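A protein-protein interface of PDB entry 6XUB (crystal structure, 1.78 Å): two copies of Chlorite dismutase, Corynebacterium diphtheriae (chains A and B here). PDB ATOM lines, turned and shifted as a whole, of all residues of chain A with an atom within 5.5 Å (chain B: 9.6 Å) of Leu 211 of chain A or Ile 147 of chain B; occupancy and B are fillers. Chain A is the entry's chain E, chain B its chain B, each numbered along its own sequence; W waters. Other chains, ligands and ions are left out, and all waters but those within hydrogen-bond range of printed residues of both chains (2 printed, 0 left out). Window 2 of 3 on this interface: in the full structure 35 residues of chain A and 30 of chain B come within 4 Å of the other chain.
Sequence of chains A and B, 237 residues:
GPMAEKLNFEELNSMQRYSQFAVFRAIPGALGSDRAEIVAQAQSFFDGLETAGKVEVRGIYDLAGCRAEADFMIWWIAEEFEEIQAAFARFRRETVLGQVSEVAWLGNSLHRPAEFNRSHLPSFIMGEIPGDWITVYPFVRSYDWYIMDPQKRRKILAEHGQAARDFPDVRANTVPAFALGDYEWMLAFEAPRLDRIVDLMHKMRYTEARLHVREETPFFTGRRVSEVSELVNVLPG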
ATOM      1  N   SER A 142      23.034   8.027  -1.156  1.00  0.00           N
ATOM      2  CA  SER A 142      21.774   8.478  -1.731  1.00  0.00           C
ATOM      3  C   SER A 142      21.110   7.372  -2.547  1.00  0.00           C
ATOM      4  O   SER A 142      21.761   6.443  -3.043  1.00  0.00           O
ATOM      5  CB  SER A 142      21.999   9.689  -2.628  1.00  0.00           C
ATOM      6  OG  SER A 142      22.935   9.382  -3.617  1.00  0.00           O
ATOM      7  N   ARG A 205      35.100  16.611   3.177  1.00  0.00           N
ATOM      8  CA  ARG A 205      33.829  17.295   2.913  1.00  0.00           C
ATOM      9  C   ARG A 205      33.879  18.044   1.591  1.00  0.00           C
ATOM     10  O   ARG A 205      32.830  18.294   0.990  1.00  0.00           O
ATOM     11  CB  ARG A 205      33.455  18.296   4.038  1.00  0.00           C
ATOM     12  CG  ARG A 205      33.018  17.670   5.355  1.00  0.00           C
ATOM     13  CD  ARG A 205      31.789  16.815   5.152  1.00  0.00           C
ATOM     14  NE  ARG A 205      30.963  16.555   6.334  1.00  0.00           N
ATOM     15  CZ  ARG A 205      31.019  15.465   7.089  1.00  0.00           C
ATOM     16  NH1 ARG A 205      31.906  14.512   6.855  1.00  0.00           N
ATOM     17  NH2 ARG A 205      30.157  15.313   8.084  1.00  0.00           N
ATOM     18  N   TYR A 206      35.077  18.380   1.114  1.00  0.00           N
ATOM     19  CA  TYR A 206      35.245  19.170  -0.106  1.00  0.00           C
ATOM     20  C   TYR A 206      35.256  18.282  -1.338  1.00  0.00           C
ATOM     21  O   TYR A 206      36.207  18.312  -2.125  1.00  0.00           O
ATOM     22  CB  TYR A 206      36.549  19.973  -0.001  1.00  0.00           C
ATOM     23  CG  TYR A 206      36.462  21.044   1.036  1.00  0.00           C
ATOM     24  CD1 TYR A 206      36.527  20.730   2.391  1.00  0.00           C
ATOM     25  CD2 TYR A 206      36.255  22.371   0.676  1.00  0.00           C
ATOM     26  CE1 TYR A 206      36.403  21.718   3.359  1.00  0.00           C
ATOM     27  CE2 TYR A 206      36.136  23.364   1.644  1.00  0.00           C
ATOM     28  CZ  TYR A 206      36.222  23.028   2.983  1.00  0.00           C
ATOM     29  OH  TYR A 206      36.091  23.999   3.965  1.00  0.00           O
ATOM     30  N   THR A 207      34.234  17.437  -1.490  1.00  0.00           N
ATOM     31  CA  THR A 207      34.193  16.446  -2.550  1.00  0.00           C
ATOM     32  C   THR A 207      32.780  16.376  -3.110  1.00  0.00           C
ATOM     33  O   THR A 207      31.801  16.575  -2.388  1.00  0.00           O
ATOM     34  CB  THR A 207      34.610  15.049  -2.053  1.00  0.00           C
ATOM     35  OG1 THR A 207      33.857  14.704  -0.895  1.00  0.00           O
ATOM     36  CG2 THR A 207      36.116  14.996  -1.703  1.00  0.00           C
ATOM     37  N   GLU A 208      32.682  16.083  -4.410  1.00  0.00           N
ATOM     38  CA  GLU A 208      31.371  15.898  -5.030  1.00  0.00           C
ATOM     39  C   GLU A 208      30.623  14.697  -4.448  1.00  0.00           C
ATOM     40  O   GLU A 208      29.390  14.666  -4.509  1.00  0.00           O
ATOM     41  CB  GLU A 208      31.536  15.739  -6.551  1.00  0.00           C
ATOM     42  CG  GLU A 208      30.231  15.504  -7.295  1.00  0.00           C
ATOM     43  CD  GLU A 208      30.352  15.736  -8.812  1.00  0.00           C
ATOM     44  OE1 GLU A 208      31.469  16.008  -9.301  1.00  0.00           O
ATOM     45  OE2 GLU A 208      29.325  15.645  -9.513  1.00  0.00           O
ATOM     46  N   ALA A 209      31.345  13.723  -3.887  1.00  0.00           N
ATOM     47  CA  ALA A 209      30.715  12.567  -3.275  1.00  0.00           C
ATOM     48  C   ALA A 209      29.736  12.946  -2.167  1.00  0.00           C
ATOM     49  O   ALA A 209      28.784  12.201  -1.911  1.00  0.00           O
ATOM     50  CB  ALA A 209      31.780  11.644  -2.716  1.00  0.00           C
ATOM     51  N   ARG A 210      29.983  14.066  -1.468  1.00  0.00           N
ATOM     52  CA  ARG A 210      29.116  14.511  -0.386  1.00  0.00           C
ATOM     53  C   ARG A 210      27.714  14.796  -0.870  1.00  0.00           C
ATOM     54  O   ARG A 210      26.784  14.844  -0.055  1.00  0.00           O
ATOM     55  CB  ARG A 210      29.727  15.756   0.277  1.00  0.00           C
ATOM     56  CG  ARG A 210      31.051  15.450   0.988  1.00  0.00           C
ATOM     57  CD  ARG A 210      30.869  14.412   2.118  1.00  0.00           C
ATOM     58  NE  ARG A 210      29.847  14.852   3.056  1.00  0.00           N
ATOM     59  CZ  ARG A 210      29.402  14.141   4.083  1.00  0.00           C
ATOM     60  NH1 ARG A 210      29.909  12.947   4.326  1.00  0.00           N
ATOM     61  NH2 ARG A 210      28.442  14.630   4.876  1.00  0.00           N
ATOM     62  N   LEU A 211      27.533  14.970  -2.177  1.00  0.00           N
ATOM     63  CA  LEU A 211      26.206  15.221  -2.734  1.00  0.00           C
ATOM     64  C   LEU A 211      25.387  13.943  -2.885  1.00  0.00           C
ATOM     65  O   LEU A 211      24.253  13.999  -3.382  1.00  0.00           O
ATOM     66  CB  LEU A 211      26.339  15.929  -4.085  1.00  0.00           C
ATOM     67  CG  LEU A 211      27.118  17.247  -4.067  1.00  0.00           C
ATOM     68  CD1 LEU A 211      27.292  17.754  -5.521  1.00  0.00           C
ATOM     69  CD2 LEU A 211      26.455  18.293  -3.184  1.00  0.00           C
ATOM     70  N   HIS A 212      25.912  12.807  -2.440  1.00  0.00           N
ATOM     71  CA  HIS A 212      25.282  11.496  -2.602  1.00  0.00           C
ATOM     72  C   HIS A 212      25.382  10.679  -1.327  1.00  0.00           C
ATOM     73  O   HIS A 212      25.795   9.512  -1.341  1.00  0.00           O
ATOM     74  CB  HIS A 212      25.902  10.794  -3.813  1.00  0.00           C
ATOM     75  CG  HIS A 212      25.742  11.595  -5.060  1.00  0.00           C
ATOM     76  ND1 HIS A 212      26.738  12.409  -5.555  1.00  0.00           N
ATOM     77  CD2 HIS A 212      24.657  11.804  -5.839  1.00  0.00           C
ATOM     78  CE1 HIS A 212      26.287  13.037  -6.629  1.00  0.00           C
ATOM     79  NE2 HIS A 212      25.022  12.705  -6.809  1.00  0.00           N
ATOM     80  N   VAL A 213      24.898  11.280  -0.234  1.00  0.00           N
ATOM     81  CA  VAL A 213      24.923  10.725   1.117  1.00  0.00           C
ATOM     82  C   VAL A 213      23.547  10.842   1.762  1.00  0.00           C
ATOM     83  O   VAL A 213      22.909  11.900   1.698  1.00  0.00           O
ATOM     84  CB  VAL A 213      25.964  11.477   1.988  1.00  0.00           C
ATOM     85  CG1 VAL A 213      25.997  10.952   3.386  1.00  0.00           C
ATOM     86  CG2 VAL A 213      27.336  11.334   1.340  1.00  0.00           C
ATOM     87  N   GLU B 115      38.333  28.994   7.675  1.00  0.00           N
ATOM     88  CA  GLU B 115      38.612  28.762   6.263  1.00  0.00           C
ATOM     89  C   GLU B 115      39.014  30.050   5.562  1.00  0.00           C
ATOM     90  O   GLU B 115      39.964  30.066   4.765  1.00  0.00           O
ATOM     91  CB  GLU B 115      37.388  28.132   5.564  1.00  0.00           C
ATOM     92  CG  GLU B 115      37.587  28.004   4.071  1.00  0.00           C
ATOM     93  CD  GLU B 115      36.442  27.281   3.381  1.00  0.00           C
ATOM     94  OE1 GLU B 115      35.354  27.103   3.997  1.00  0.00           O
ATOM     95  OE2 GLU B 115      36.656  26.890   2.222  1.00  0.00           O
ATOM     96  N   ARG B 141      26.256  21.330   8.587  1.00  0.00           N
ATOM     97  CA  ARG B 141      25.929  22.067   7.379  1.00  0.00           C
ATOM     98  C   ARG B 141      25.211  21.191   6.354  1.00  0.00           C
ATOM     99  O   ARG B 141      25.253  19.963   6.403  1.00  0.00           O
ATOM    100  CB  ARG B 141      27.217  22.600   6.746  1.00  0.00           C
ATOM    101  CG  ARG B 141      27.838  23.775   7.468  1.00  0.00           C
ATOM    102  CD  ARG B 141      27.082  25.045   7.059  1.00  0.00           C
ATOM    103  NE  ARG B 141      27.575  26.215   7.760  1.00  0.00           N
ATOM    104  CZ  ARG B 141      26.831  27.261   8.102  1.00  0.00           C
ATOM    105  NH1 ARG B 141      25.522  27.267   7.831  1.00  0.00           N
ATOM    106  NH2 ARG B 141      27.375  28.259   8.809  1.00  0.00           N
ATOM    107  N   SER B 142      24.598  21.854   5.377  1.00  0.00           N
ATOM    108  CA  SER B 142      24.024  21.167   4.217  1.00  0.00           C
ATOM    109  C   SER B 142      25.092  20.331   3.500  1.00  0.00           C
ATOM    110  O   SER B 142      26.285  20.608   3.565  1.00  0.00           O
ATOM    111  CB  SER B 142      23.433  22.186   3.255  1.00  0.00           C
ATOM    112  OG  SER B 142      24.390  23.131   2.869  1.00  0.00           O
ATOM    113  N   TYR B 143      24.642  19.294   2.786  1.00  0.00           N
ATOM    114  CA  TYR B 143      25.602  18.430   2.105  1.00  0.00           C
ATOM    115  C   TYR B 143      26.432  19.195   1.085  1.00  0.00           C
ATOM    116  O   TYR B 143      27.589  18.825   0.825  1.00  0.00           O
ATOM    117  CB  TYR B 143      24.891  17.282   1.382  1.00  0.00           C
ATOM    118  CG  TYR B 143      24.381  16.213   2.277  1.00  0.00           C
ATOM    119  CD1 TYR B 143      25.254  15.442   3.044  1.00  0.00           C
ATOM    120  CD2 TYR B 143      23.022  15.983   2.389  1.00  0.00           C
ATOM    121  CE1 TYR B 143      24.768  14.462   3.864  1.00  0.00           C
ATOM    122  CE2 TYR B 143      22.541  15.029   3.234  1.00  0.00           C
ATOM    123  CZ  TYR B 143      23.399  14.255   3.922  1.00  0.00           C
ATOM    124  OH  TYR B 143      22.891  13.298   4.713  1.00  0.00           O
ATOM    125  N   ASP B 144      25.865  20.245   0.486  1.00  0.00           N
ATOM    126  CA  ASP B 144      26.518  20.972  -0.604  1.00  0.00           C
ATOM    127  C   ASP B 144      27.462  22.082  -0.132  1.00  0.00           C
ATOM    128  O   ASP B 144      28.104  22.729  -0.962  1.00  0.00           O
ATOM    129  CB  ASP B 144      25.457  21.544  -1.549  1.00  0.00           C
ATOM    130  CG  ASP B 144      24.689  22.729  -0.955  1.00  0.00           C
ATOM    131  OD1 ASP B 144      24.943  23.126   0.204  1.00  0.00           O
ATOM    132  OD2 ASP B 144      23.824  23.276  -1.679  1.00  0.00           O
ATOM    133  N   TRP B 145      27.617  22.264   1.180  1.00  0.00           N
ATOM    134  CA  TRP B 145      28.261  23.463   1.716  1.00  0.00           C
ATOM    135  C   TRP B 145      29.741  23.558   1.362  1.00  0.00           C
ATOM    136  O   TRP B 145      30.223  24.627   0.971  1.00  0.00           O
ATOM    137  CB  TRP B 145      28.080  23.473   3.240  1.00  0.00           C
ATOM    138  CG  TRP B 145      28.766  24.582   3.959  1.00  0.00           C
ATOM    139  CD1 TRP B 145      29.812  24.465   4.844  1.00  0.00           C
ATOM    140  CD2 TRP B 145      28.447  25.976   3.892  1.00  0.00           C
ATOM    141  NE1 TRP B 145      30.175  25.702   5.301  1.00  0.00           N
ATOM    142  CE2 TRP B 145      29.325  26.644   4.767  1.00  0.00           C
ATOM    143  CE3 TRP B 145      27.478  26.724   3.198  1.00  0.00           C
ATOM    144  CZ2 TRP B 145      29.289  28.025   4.946  1.00  0.00           C
ATOM    145  CZ3 TRP B 145      27.432  28.098   3.391  1.00  0.00           C
ATOM    146  CH2 TRP B 145      28.334  28.737   4.255  1.00  0.00           C
ATOM    147  N   TYR B 146      30.482  22.476   1.541  1.00  0.00           N
ATOM    148  CA  TYR B 146      31.944  22.505   1.380  1.00  0.00           C
ATOM    149  C   TYR B 146      32.389  22.361  -0.065  1.00  0.00           C
ATOM    150  O   TYR B 146      33.445  22.908  -0.436  1.00  0.00           O
ATOM    151  CB  TYR B 146      32.583  21.398   2.213  1.00  0.00           C
ATOM    152  CG  TYR B 146      32.147  21.448   3.662  1.00  0.00           C
ATOM    153  CD1 TYR B 146      32.845  22.204   4.606  1.00  0.00           C
ATOM    154  CD2 TYR B 146      31.024  20.747   4.083  1.00  0.00           C
ATOM    155  CE1 TYR B 146      32.434  22.252   5.937  1.00  0.00           C
ATOM    156  CE2 TYR B 146      30.601  20.794   5.397  1.00  0.00           C
ATOM    157  CZ  TYR B 146      31.303  21.542   6.319  1.00  0.00           C
ATOM    158  OH  TYR B 146      30.856  21.547   7.612  1.00  0.00           O
ATOM    159  N   ILE B 147      31.616  21.640  -0.892  1.00  0.00           N
ATOM    160  CA  ILE B 147      31.983  21.500  -2.305  1.00  0.00           C
ATOM    161  C   ILE B 147      31.538  22.706  -3.104  1.00  0.00           C
ATOM    162  O   ILE B 147      32.008  22.906  -4.226  1.00  0.00           O
ATOM    163  CB  ILE B 147      31.415  20.191  -2.881  1.00  0.00           C
ATOM    164  CG1 ILE B 147      32.018  19.899  -4.264  1.00  0.00           C
ATOM    165  CG2 ILE B 147      29.907  20.219  -2.950  1.00  0.00           C
ATOM    166  CD1 ILE B 147      33.561  19.916  -4.318  1.00  0.00           C
ATOM    167  N   MET B 148      30.660  23.530  -2.552  1.00  0.00           N
ATOM    168  CA  MET B 148      30.242  24.753  -3.228  1.00  0.00           C
ATOM    169  C   MET B 148      31.461  25.578  -3.634  1.00  0.00           C
ATOM    170  O   MET B 148      32.520  25.515  -3.001  1.00  0.00           O
ATOM    171  CB  MET B 148      29.333  25.534  -2.267  1.00  0.00           C
ATOM    172  CG  MET B 148      29.184  27.020  -2.506  1.00  0.00           C
ATOM    173  SD  MET B 148      28.242  27.836  -1.181  1.00  0.00           S
ATOM    174  CE  MET B 148      27.010  26.639  -0.745  1.00  0.00           C
ATOM    175  N   ASP B 149      31.295  26.381  -4.681  1.00  0.00           N
ATOM    176  CA  ASP B 149      32.376  27.241  -5.151  1.00  0.00           C
ATOM    177  C   ASP B 149      32.914  28.090  -3.998  1.00  0.00           C
ATOM    178  O   ASP B 149      32.123  28.761  -3.314  1.00  0.00           O
ATOM    179  CB  ASP B 149      31.866  28.163  -6.254  1.00  0.00           C
ATOM    180  CG  ASP B 149      32.983  28.873  -6.970  1.00  0.00           C
ATOM    181  OD1 ASP B 149      32.840  30.081  -7.252  1.00  0.00           O
ATOM    182  OD2 ASP B 149      34.010  28.219  -7.244  1.00  0.00           O
ATOM    183  N   PRO B 150      34.236  28.138  -3.780  1.00  0.00           N
ATOM    184  CA  PRO B 150      34.719  28.865  -2.595  1.00  0.00           C
ATOM    185  C   PRO B 150      34.307  30.327  -2.591  1.00  0.00           C
ATOM    186  O   PRO B 150      33.933  30.849  -1.536  1.00  0.00           O
ATOM    187  CB  PRO B 150      36.244  28.671  -2.658  1.00  0.00           C
ATOM    188  CG  PRO B 150      36.423  27.386  -3.448  1.00  0.00           C
ATOM    189  CD  PRO B 150      35.331  27.429  -4.478  1.00  0.00           C
ATOM    190  N   GLN B 151      34.296  30.984  -3.753  1.00  0.00           N
ATOM    191  CA  GLN B 151      33.875  32.384  -3.818  1.00  0.00           C
ATOM    192  C   GLN B 151      32.476  32.557  -3.237  1.00  0.00           C
ATOM    193  O   GLN B 151      32.176  33.569  -2.585  1.00  0.00           O
ATOM    194  CB  GLN B 151      33.922  32.855  -5.281  1.00  0.00           C
ATOM    195  CG  GLN B 151      33.353  34.256  -5.564  1.00  0.00           C
ATOM    196  CD  GLN B 151      33.397  34.628  -7.063  1.00  0.00           C
ATOM    197  OE1 GLN B 151      33.632  33.778  -7.920  1.00  0.00           O
ATOM    198  NE2 GLN B 151      33.162  35.909  -7.366  1.00  0.00           N
ATOM    199  N   LYS B 152      31.618  31.564  -3.448  1.00  0.00           N
ATOM    200  CA  LYS B 152      30.240  31.639  -2.991  1.00  0.00           C
ATOM    201  C   LYS B 152      30.168  31.427  -1.491  1.00  0.00           C
ATOM    202  O   LYS B 152      29.466  32.159  -0.787  1.00  0.00           O
ATOM    203  CB  LYS B 152      29.393  30.606  -3.724  1.00  0.00           C
ATOM    204  CG  LYS B 152      28.656  31.170  -4.917  1.00  0.00           C
ATOM    205  CD  LYS B 152      27.345  31.796  -4.481  1.00  0.00           C
ATOM    206  CE  LYS B 152      27.225  33.231  -4.982  1.00  0.00           C
ATOM    207  NZ  LYS B 152      26.114  33.975  -4.310  1.00  0.00           N
ATOM    208  N   ARG B 153      30.919  30.447  -0.983  1.00  0.00           N
ATOM    209  CA  ARG B 153      30.896  30.186   0.451  1.00  0.00           C
ATOM    210  C   ARG B 153      31.523  31.358   1.193  1.00  0.00           C
ATOM    211  O   ARG B 153      31.049  31.745   2.265  1.00  0.00           O
ATOM    212  CB  ARG B 153      31.606  28.864   0.764  1.00  0.00           C
ATOM    213  CG  ARG B 153      31.420  28.364   2.218  1.00  0.00           C
ATOM    214  CD  ARG B 153      32.099  26.980   2.535  1.00  0.00           C
ATOM    215  NE  ARG B 153      33.395  26.820   1.898  1.00  0.00           N
ATOM    216  CZ  ARG B 153      33.557  26.398   0.649  1.00  0.00           C
ATOM    217  NH1 ARG B 153      32.491  26.034  -0.081  1.00  0.00           N
ATOM    218  NH2 ARG B 153      34.776  26.323   0.133  1.00  0.00           N
ATOM    219  N   HIS B 212      21.782  26.636   4.250  1.00  0.00           N
ATOM    220  CA  HIS B 212      22.841  25.611   4.157  1.00  0.00           C
ATOM    221  C   HIS B 212      23.064  24.960   5.510  1.00  0.00           C
ATOM    222  O   HIS B 212      24.196  24.767   5.979  1.00  0.00           O
ATOM    223  CB  HIS B 212      24.107  26.236   3.564  1.00  0.00           C
ATOM    224  CG  HIS B 212      23.890  26.742   2.163  1.00  0.00           C
ATOM    225  ND1 HIS B 212      23.889  25.909   1.063  1.00  0.00           N
ATOM    226  CD2 HIS B 212      23.583  27.976   1.695  1.00  0.00           C
ATOM    227  CE1 HIS B 212      23.626  26.613  -0.024  1.00  0.00           C
ATOM    228  NE2 HIS B 212      23.424  27.868   0.332  1.00  0.00           N
ATOM    229  N   ARG B 214      21.651  21.693   8.154  1.00  0.00           N
ATOM    230  CA  ARG B 214      20.979  20.408   8.264  1.00  0.00           C
ATOM    231  C   ARG B 214      20.599  20.039   9.687  1.00  0.00           C
ATOM    232  O   ARG B 214      19.563  19.425   9.895  1.00  0.00           O
ATOM    233  CB  ARG B 214      21.876  19.280   7.717  1.00  0.00           C
ATOM    234  CG  ARG B 214      21.655  18.938   6.288  1.00  0.00           C
ATOM    235  CD  ARG B 214      22.199  17.542   6.011  1.00  0.00           C
ATOM    236  NE  ARG B 214      23.653  17.451   6.083  1.00  0.00           N
ATOM    237  CZ  ARG B 214      24.313  16.450   6.647  1.00  0.00           C
ATOM    238  NH1 ARG B 214      23.647  15.491   7.268  1.00  0.00           N
ATOM    239  NH2 ARG B 214      25.637  16.440   6.614  1.00  0.00           N
HETATM  240  O   HOH W   1      30.265  19.755   0.592  1.00  0.00           O
HETATM  241  O   HOH W   2      28.929  17.624   3.125  1.00  0.00           O
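OE1 of Glu 115 of chain B lies within hydrogen-bond range of OH of Tyr 206 of chain A (3.2 Å). OH of Tyr 143 of chain B lies close to O of Val 213 of chain A (3.3 Å).
The backbone carbonyl oxygen (O) of Met 148 of chain B sits at hydrogen-bond distance from the guanidinium group (NH1) of Arg 153 of chain B, at 3.0 Å. The side-chain carboxylate of Glu 115 of chain B lies within salt-bridge range of the guanidinium group of Arg 153 of chain B (2.9 Å). The side-chain hydroxyl of Ser 142 of chain B is in hydrogen-bond range of the side-chain carboxylate of Asp 144 of chain B (2.7 Å). The backbone carbonyl oxygen (O) of Tyr 146 of chain B is in hydrogen-bond range of the guanidinium group (NH1) of Arg 153 of chain B (3.3 Å). O of Trp 145 of chain B lies within hydrogen-bond range of NH1 of Arg 153 of chain B (2.9 Å). The guanidinium group of Arg 214 of chain B lies within hydrogen-bond range of the side-chain hydroxyl of Tyr 143 of chain B, 3.5 Å away.
Among the printed residues, merely in contact across the chains: Tyr 206 of chain A with Tyr 146 of chain B (3.1 Å), Arg 205 of chain A with Tyr 146 of chain B (3.3 Å), Arg 210 of chain A with Tyr 143 of chain B (3.4 Å), Tyr 206 of chain A with Arg 153 of chain B (3.6 Å), Thr 207 of chain A with Ile 147 of chain B (3.7 Å), Leu 211 of chain A with Asp 144 of chain B (3.7 Å), Arg 210 of chain A with Arg 214 of chain B (3.8 Å), Tyr 206 of chain A with Ile 147 of chain B (3.8 Å), Glu 208 of chain A with Ile 147 of chain B (3.9 Å) and Leu 211 of chain A with Ile 147 of chain B (3.96 Å).
Leu 211 of chain A touches two residues of chain B. Ile 147 of chain B touches four residues of chain A. His 212 of chain A touches none of the printed residues of chain B. Printed residues of chain B within 4 Å of Glu 208 of chain A: Ile 147. Printed residues of chain B within 4 Å of Thr 207 of chain A: Ile 147. Of the printed residues of chain A, Glu 115 of chain B touches Tyr 206 (3.2 Å). Of the printed residues of chain A, Tyr 143 of chain B touches Arg 210 and Val 213. Of the printed residues of chain A, Asp 144 of chain B touches Leu 211. Arg 141 of chain B touches none of the printed residues of chain A. Lys 152 of chain B touches none of the printed residues of chain A. The nearest residue of chain A that does not touch Ile 147 of chain B is Arg 205 of chain A (4.03 Å).
Printed residues of chain A that touch a printed residue of chain B: Arg 205, Tyr 206, Thr 207, Glu 208, Arg 210, Leu 211 and Val 213. Hydrophobic or aromatic side chains of chain A within 4 Å of the printed part of chain B: Tyr 206, Leu 211 and Val 213. Printed residues of chain B that touch a printed residue of chain A: Glu 115, Tyr 143, Asp 144, Tyr 146, Ile 147, Arg 153 and Arg 214. Among the printed residues, no Asp or Glu carboxylate lies within 4 Å of a Lys or Arg side-chain nitrogen of the other chain.
2 positions are printed for both chains. Of the 12 pairs that touch across the chains among the printed residues, none has its exchanged pair printed and touching as well.
Water W1 lies within hydrogen-bond range of N of Ile 147 of chain B (2.8 Å), O of Tyr 143 of chain B (2.8 Å), N of Tyr 146 of chain B (2.9 Å) and O of Arg 205 of chain A (3.0 Å). Water W2 bridges NE of Arg 210 of chain A and O of Tyr 143 of chain B.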
